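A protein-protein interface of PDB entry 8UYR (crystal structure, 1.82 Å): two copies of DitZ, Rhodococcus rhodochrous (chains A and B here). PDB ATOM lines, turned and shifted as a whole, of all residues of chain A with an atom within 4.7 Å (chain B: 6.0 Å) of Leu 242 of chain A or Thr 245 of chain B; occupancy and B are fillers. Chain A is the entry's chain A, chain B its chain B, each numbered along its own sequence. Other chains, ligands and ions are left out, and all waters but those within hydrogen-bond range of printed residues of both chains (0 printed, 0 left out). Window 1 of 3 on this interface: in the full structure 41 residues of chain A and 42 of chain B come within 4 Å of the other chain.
The indole nitrogen (NE1) of Trp 278 of chain B lies within hydrogen-bond range of the side-chain hydroxyl (OG1) of Thr 249 of chain B (2.8 Å).
The side-chain hydroxyl of Thr 249 of chain B is in hydrogen-bond range of the backbone carbonyl oxygen of Thr 245 of chain B, 2.7 Å away.
Printed residues of chain B within 4 Å of Leu 242 of chain A: Thr 245 (3.99 Å) and Trp 278 (3.9 Å).
Of the printed residues of chain A, Thr 245 of chain B touches Leu 239 (3.8 Å) and Leu 242 (3.99 Å).
Of the printed residues of chain B, Leu 239 of chain A touches Thr 245 (3.8 Å), Ile 246 (3.8 Å) and Thr 249 (3.5 Å).
Of the printed residues of chain A, Thr 249 of chain B touches Met 238 (3.8 Å) and Leu 239 (3.5 Å).
Of the printed residues of chain B, Thr 245 of chain A touches Leu 242.
Printed residues of chain A within 4 Å of Arg 281 of chain B: Met 238 (3.7 Å) and Pro 241 (3.3 Å).
Of the printed residues of chain B, Pro 241 of chain A touches Arg 281 (3.3 Å).
The nearest printed residue of chain A that does not touch Thr 245 of chain B is Ile 243 of chain A (5.3 Å).
The nearest printed residue of chain A that does not touch Ile 246 of chain B is Ile 243 of chain A (5.1 Å).
Leu 242 of chain A touches Thr 245 of chain B, and with the chains exchanged Thr 245 of chain A touches Leu 242 of chain B.
Of the 9 pairs that touch across the chains among the printed residues, 2 have their exchanged pair printed and touching as well.
Thr 249 of chain B touches Met 238 of chain A (CG2 to CB, 3.8 Å).
Arg 281 of chain B touches Met 238 of chain A (CG to CE, 3.7 Å).
O of Thr 245 of chain B touches CD2 of Leu 239 of chain A, at 3.8 Å.
Leu 239 of chain A touches Ile 246 of chain B (CD2 to CA, 3.8 Å).
CD2 of Leu 239 of chain A touches OG1 of Thr 249 of chain B, 3.5 Å away.
Pro 241 of chain A touches Arg 281 of chain B.
Leu 242 of chain A touches Thr 245 of chain B.
CD1 of Leu 242 of chain A touches CD1 of Trp 278 of chain B (3.9 Å).
Thr 245 of chain A touches Leu 242 of chain B.
Of the 14 printed residues of chain B, 6 touch a printed residue of chain A.
Hydrophobic or aromatic side chains of chain B within 4 Å of the printed part of chain A: Leu 242 and Trp 278.
Hydrophobic or aromatic side chains of chain A within 4 Å of the printed part of chain B: Met 238, Leu 239, Pro 241 and Leu 242.
Among the printed residues, 9 pairs touch across the chains.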
ATOM      1  N   MET A 238     -14.096  16.199  -4.938  1.00  0.00           N
ATOM      2  CA  MET A 238     -14.898  15.608  -3.874  1.00  0.00           C
ATOM      3  C   MET A 238     -15.137  14.118  -4.110  1.00  0.00           C
ATOM      4  O   MET A 238     -15.093  13.327  -3.165  1.00  0.00           O
ATOM      5  CB  MET A 238     -16.226  16.352  -3.723  1.00  0.00           C
ATOM      6  CG  MET A 238     -16.094  17.759  -3.108  1.00  0.00           C
ATOM      7  SD  MET A 238     -15.414  17.717  -1.430  1.00  0.00           S
ATOM      8  CE  MET A 238     -16.336  16.311  -0.805  1.00  0.00           C
ATOM      9  N   LEU A 239     -15.397  13.706  -5.355  1.00  0.00           N
ATOM     10  CA  LEU A 239     -15.759  12.305  -5.564  1.00  0.00           C
ATOM     11  C   LEU A 239     -14.541  11.400  -5.656  1.00  0.00           C
ATOM     12  O   LEU A 239     -14.566  10.277  -5.141  1.00  0.00           O
ATOM     13  CB  LEU A 239     -16.582  12.136  -6.835  1.00  0.00           C
ATOM     14  CG  LEU A 239     -17.978  12.734  -6.876  1.00  0.00           C
ATOM     15  CD1 LEU A 239     -18.570  12.297  -8.201  1.00  0.00           C
ATOM     16  CD2 LEU A 239     -18.802  12.237  -5.689  1.00  0.00           C
ATOM     17  N   THR A 240     -13.481  11.861  -6.329  1.00  0.00           N
ATOM     18  CA  THR A 240     -12.371  10.980  -6.694  1.00  0.00           C
ATOM     19  C   THR A 240     -11.874  10.093  -5.554  1.00  0.00           C
ATOM     20  O   THR A 240     -11.684   8.886  -5.786  1.00  0.00           O
ATOM     21  CB  THR A 240     -11.221  11.813  -7.287  1.00  0.00           C
ATOM     22  OG1 THR A 240     -11.642  12.402  -8.524  1.00  0.00           O
ATOM     23  CG2 THR A 240      -9.983  10.919  -7.561  1.00  0.00           C
ATOM     24  N   PRO A 241     -11.660  10.580  -4.328  1.00  0.00           N
ATOM     25  CA  PRO A 241     -11.145   9.698  -3.274  1.00  0.00           C
ATOM     26  C   PRO A 241     -12.199   9.007  -2.423  1.00  0.00           C
ATOM     27  O   PRO A 241     -11.829   8.337  -1.454  1.00  0.00           O
ATOM     28  CB  PRO A 241     -10.324  10.663  -2.417  1.00  0.00           C
ATOM     29  CG  PRO A 241     -11.104  11.937  -2.490  1.00  0.00           C
ATOM     30  CD  PRO A 241     -11.673  11.989  -3.881  1.00  0.00           C
ATOM     31  N   LEU A 242     -13.483   9.140  -2.738  1.00  0.00           N
ATOM     32  CA  LEU A 242     -14.544   8.586  -1.905  1.00  0.00           C
ATOM     33  C   LEU A 242     -15.215   7.365  -2.527  1.00  0.00           C
ATOM     34  O   LEU A 242     -16.232   6.895  -2.002  1.00  0.00           O
ATOM     35  CB  LEU A 242     -15.580   9.672  -1.615  1.00  0.00           C
ATOM     36  CG  LEU A 242     -15.066  10.903  -0.855  1.00  0.00           C
ATOM     37  CD1 LEU A 242     -16.190  11.903  -0.684  1.00  0.00           C
ATOM     38  CD2 LEU A 242     -14.469  10.513   0.510  1.00  0.00           C
ATOM     39  N   ILE A 243     -14.677   6.838  -3.627  1.00  0.00           N
ATOM     40  CA  ILE A 243     -15.357   5.774  -4.359  1.00  0.00           C
ATOM     41  C   ILE A 243     -14.441   4.570  -4.557  1.00  0.00           C
ATOM     42  O   ILE A 243     -14.561   3.840  -5.545  1.00  0.00           O
ATOM     43  CB  ILE A 243     -15.894   6.291  -5.706  1.00  0.00           C
ATOM     44  CG1 ILE A 243     -14.772   6.899  -6.542  1.00  0.00           C
ATOM     45  CG2 ILE A 243     -17.026   7.324  -5.482  1.00  0.00           C
ATOM     46  CD1 ILE A 243     -15.181   7.136  -7.983  1.00  0.00           C
ATOM     47  N   SER A 244     -13.532   4.340  -3.608  1.00  0.00           N
ATOM     48  CA  SER A 244     -12.757   3.102  -3.598  1.00  0.00           C
ATOM     49  C   SER A 244     -13.634   1.874  -3.426  1.00  0.00           C
ATOM     50  O   SER A 244     -13.146   0.752  -3.604  1.00  0.00           O
ATOM     51  CB  SER A 244     -11.727   3.142  -2.471  1.00  0.00           C
ATOM     52  OG  SER A 244     -10.780   4.172  -2.686  1.00  0.00           O
ATOM     53  N   THR A 245     -14.893   2.070  -3.036  1.00  0.00           N
ATOM     54  CA  THR A 245     -15.863   0.985  -2.964  1.00  0.00           C
ATOM     55  C   THR A 245     -15.922   0.185  -4.261  1.00  0.00           C
ATOM     56  O   THR A 245     -16.151  -1.029  -4.230  1.00  0.00           O
ATOM     57  CB  THR A 245     -17.246   1.563  -2.642  1.00  0.00           C
ATOM     58  OG1 THR A 245     -17.149   2.408  -1.487  1.00  0.00           O
ATOM     59  CG2 THR A 245     -18.246   0.452  -2.357  1.00  0.00           C
ATOM     60  N   LEU B 242     -24.496   1.844  -2.321  1.00  0.00           N
ATOM     61  CA  LEU B 242     -23.363   2.352  -1.557  1.00  0.00           C
ATOM     62  C   LEU B 242     -22.732   3.605  -2.167  1.00  0.00           C
ATOM     63  O   LEU B 242     -21.694   4.060  -1.674  1.00  0.00           O
ATOM     64  CB  LEU B 242     -22.307   1.252  -1.388  1.00  0.00           C
ATOM     65  CG  LEU B 242     -22.689  -0.085  -0.727  1.00  0.00           C
ATOM     66  CD1 LEU B 242     -21.517  -1.068  -0.799  1.00  0.00           C
ATOM     67  CD2 LEU B 242     -23.132   0.090   0.713  1.00  0.00           C
ATOM     68  N   ILE B 243     -23.339   4.191  -3.204  1.00  0.00           N
ATOM     69  CA  ILE B 243     -22.721   5.299  -3.932  1.00  0.00           C
ATOM     70  C   ILE B 243     -23.649   6.510  -3.999  1.00  0.00           C
ATOM     71  O   ILE B 243     -23.686   7.227  -5.008  1.00  0.00           O
ATOM     72  CB  ILE B 243     -22.313   4.858  -5.347  1.00  0.00           C
ATOM     73  CG1 ILE B 243     -23.520   4.280  -6.092  1.00  0.00           C
ATOM     74  CG2 ILE B 243     -21.189   3.814  -5.278  1.00  0.00           C
ATOM     75  CD1 ILE B 243     -23.223   3.936  -7.547  1.00  0.00           C
ATOM     76  N   SER B 244     -24.416   6.738  -2.929  1.00  0.00           N
ATOM     77  CA  SER B 244     -25.212   7.956  -2.772  1.00  0.00           C
ATOM     78  C   SER B 244     -24.345   9.200  -2.629  1.00  0.00           C
ATOM     79  O   SER B 244     -24.866  10.325  -2.691  1.00  0.00           O
ATOM     80  CB  SER B 244     -26.122   7.817  -1.548  1.00  0.00           C
ATOM     81  OG  SER B 244     -26.900   6.633  -1.638  1.00  0.00           O
ATOM     82  N   THR B 245     -23.045   9.011  -2.416  1.00  0.00           N
ATOM     83  CA  THR B 245     -22.083  10.104  -2.402  1.00  0.00           C
ATOM     84  C   THR B 245     -22.183  10.967  -3.653  1.00  0.00           C
ATOM     85  O   THR B 245     -21.992  12.184  -3.590  1.00  0.00           O
ATOM     86  CB  THR B 245     -20.677   9.517  -2.278  1.00  0.00           C
ATOM     87  OG1 THR B 245     -20.588   8.735  -1.077  1.00  0.00           O
ATOM     88  CG2 THR B 245     -19.624  10.611  -2.264  1.00  0.00           C
ATOM     89  N   ILE B 246     -22.450  10.352  -4.805  1.00  0.00           N
ATOM     90  CA  ILE B 246     -22.464  11.107  -6.056  1.00  0.00           C
ATOM     91  C   ILE B 246     -23.592  12.136  -6.047  1.00  0.00           C
ATOM     92  O   ILE B 246     -23.362  13.342  -6.208  1.00  0.00           O
ATOM     93  CB  ILE B 246     -22.576  10.156  -7.260  1.00  0.00           C
ATOM     94  CG1 ILE B 246     -21.395   9.174  -7.276  1.00  0.00           C
ATOM     95  CG2 ILE B 246     -22.647  10.959  -8.561  1.00  0.00           C
ATOM     96  CD1 ILE B 246     -21.523   8.049  -8.305  1.00  0.00           C
ATOM     97  N   ALA B 247     -24.834  11.671  -5.881  1.00  0.00           N
ATOM     98  CA  ALA B 247     -25.968  12.598  -5.946  1.00  0.00           C
ATOM     99  C   ALA B 247     -25.933  13.612  -4.815  1.00  0.00           C
ATOM    100  O   ALA B 247     -26.342  14.761  -5.009  1.00  0.00           O
ATOM    101  CB  ALA B 247     -27.287  11.826  -5.921  1.00  0.00           C
ATOM    102  N   ALA B 248     -25.438  13.219  -3.633  1.00  0.00           N
ATOM    103  CA  ALA B 248     -25.344  14.162  -2.523  1.00  0.00           C
ATOM    104  C   ALA B 248     -24.325  15.254  -2.812  1.00  0.00           C
ATOM    105  O   ALA B 248     -24.569  16.429  -2.513  1.00  0.00           O
ATOM    106  CB  ALA B 248     -24.973  13.427  -1.234  1.00  0.00           C
ATOM    107  N   THR B 249     -23.168  14.879  -3.371  1.00  0.00           N
ATOM    108  CA  THR B 249     -22.184  15.870  -3.809  1.00  0.00           C
ATOM    109  C   THR B 249     -22.775  16.800  -4.865  1.00  0.00           C
ATOM    110  O   THR B 249     -22.612  18.022  -4.786  1.00  0.00           O
ATOM    111  CB  THR B 249     -20.932  15.162  -4.345  1.00  0.00           C
ATOM    112  OG1 THR B 249     -20.364  14.344  -3.305  1.00  0.00           O
ATOM    113  CG2 THR B 249     -19.893  16.176  -4.816  1.00  0.00           C
ATOM    114  N   ASP B 250     -23.463  16.237  -5.868  1.00  0.00           N
ATOM    115  CA  ASP B 250     -24.123  17.068  -6.877  1.00  0.00           C
ATOM    116  C   ASP B 250     -25.058  18.084  -6.234  1.00  0.00           C
ATOM    117  O   ASP B 250     -25.045  19.274  -6.585  1.00  0.00           O
ATOM    118  CB  ASP B 250     -24.909  16.205  -7.869  1.00  0.00           C
ATOM    119  CG  ASP B 250     -24.028  15.280  -8.699  1.00  0.00           C
ATOM    120  OD1 ASP B 250     -22.814  15.529  -8.829  1.00  0.00           O
ATOM    121  OD2 ASP B 250     -24.580  14.305  -9.247  1.00  0.00           O
ATOM    122  N   TRP B 274     -21.795   6.234   4.293  1.00  0.00           N
ATOM    123  CA  TRP B 274     -21.177   7.105   3.302  1.00  0.00           C
ATOM    124  C   TRP B 274     -21.080   8.550   3.777  1.00  0.00           C
ATOM    125  O   TRP B 274     -20.202   9.284   3.309  1.00  0.00           O
ATOM    126  CB  TRP B 274     -21.959   7.031   1.987  1.00  0.00           C
ATOM    127  CG  TRP B 274     -23.350   7.585   2.080  1.00  0.00           C
ATOM    128  CD1 TRP B 274     -24.487   6.903   2.408  1.00  0.00           C
ATOM    129  CD2 TRP B 274     -23.748   8.939   1.835  1.00  0.00           C
ATOM    130  NE1 TRP B 274     -25.574   7.757   2.378  1.00  0.00           N
ATOM    131  CE2 TRP B 274     -25.144   9.010   2.031  1.00  0.00           C
ATOM    132  CE3 TRP B 274     -23.059  10.100   1.465  1.00  0.00           C
ATOM    133  CZ2 TRP B 274     -25.862  10.196   1.875  1.00  0.00           C
ATOM    134  CZ3 TRP B 274     -23.767  11.275   1.316  1.00  0.00           C
ATOM    135  CH2 TRP B 274     -25.158  11.317   1.521  1.00  0.00           C
ATOM    136  N   VAL B 275     -21.931   8.963   4.721  1.00  0.00           N
ATOM    137  CA  VAL B 275     -22.030  10.385   5.060  1.00  0.00           C
ATOM    138  C   VAL B 275     -20.763  10.881   5.754  1.00  0.00           C
ATOM    139  O   VAL B 275     -20.190  11.903   5.366  1.00  0.00           O
ATOM    140  CB  VAL B 275     -23.270  10.642   5.927  1.00  0.00           C
ATOM    141  CG1 VAL B 275     -23.355  12.137   6.282  1.00  0.00           C
ATOM    142  CG2 VAL B 275     -24.543  10.148   5.201  1.00  0.00           C
ATOM    143  N   PRO B 277     -17.404  10.100   5.995  1.00  0.00           N
ATOM    144  CA  PRO B 277     -16.188  10.460   5.248  1.00  0.00           C
ATOM    145  C   PRO B 277     -16.423  11.586   4.265  1.00  0.00           C
ATOM    146  O   PRO B 277     -15.511  12.376   3.991  1.00  0.00           O
ATOM    147  CB  PRO B 277     -15.814   9.160   4.519  1.00  0.00           C
ATOM    148  CG  PRO B 277     -17.096   8.376   4.445  1.00  0.00           C
ATOM    149  CD  PRO B 277     -17.793   8.698   5.743  1.00  0.00           C
ATOM    150  N   TRP B 278     -17.640  11.674   3.733  1.00  0.00           N
ATOM    151  CA  TRP B 278     -17.979  12.718   2.774  1.00  0.00           C
ATOM    152  C   TRP B 278     -18.047  14.078   3.461  1.00  0.00           C
ATOM    153  O   TRP B 278     -17.521  15.078   2.949  1.00  0.00           O
ATOM    154  CB  TRP B 278     -19.301  12.330   2.116  1.00  0.00           C
ATOM    155  CG  TRP B 278     -20.000  13.318   1.226  1.00  0.00           C
ATOM    156  CD1 TRP B 278     -19.662  13.672  -0.044  1.00  0.00           C
ATOM    157  CD2 TRP B 278     -21.219  14.006   1.523  1.00  0.00           C
ATOM    158  NE1 TRP B 278     -20.585  14.545  -0.552  1.00  0.00           N
ATOM    159  CE2 TRP B 278     -21.554  14.769   0.391  1.00  0.00           C
ATOM    160  CE3 TRP B 278     -22.055  14.054   2.641  1.00  0.00           C
ATOM    161  CZ2 TRP B 278     -22.681  15.586   0.348  1.00  0.00           C
ATOM    162  CZ3 TRP B 278     -23.187  14.852   2.591  1.00  0.00           C
ATOM    163  CH2 TRP B 278     -23.485  15.607   1.458  1.00  0.00           C
ATOM    164  N   ARG B 281     -14.532  15.337   4.178  1.00  0.00           N
ATOM    165  CA  ARG B 281     -13.882  15.918   3.011  1.00  0.00           C
ATOM    166  C   ARG B 281     -14.515  17.250   2.619  1.00  0.00           C
ATOM    167  O   ARG B 281     -13.806  18.181   2.231  1.00  0.00           O
ATOM    168  CB  ARG B 281     -13.917  14.940   1.841  1.00  0.00           C
ATOM    169  CG  ARG B 281     -13.054  15.428   0.685  1.00  0.00           C
ATOM    170  CD  ARG B 281     -12.796  14.364  -0.349  1.00  0.00           C
ATOM    171  NE  ARG B 281     -11.975  14.927  -1.416  1.00  0.00           N
ATOM    172  CZ  ARG B 281     -10.661  15.118  -1.324  1.00  0.00           C
ATOM    173  NH1 ARG B 281     -10.002  14.766  -0.216  1.00  0.00           N
ATOM    174  NH2 ARG B 281     -10.004  15.641  -2.349  1.00  0.00           N
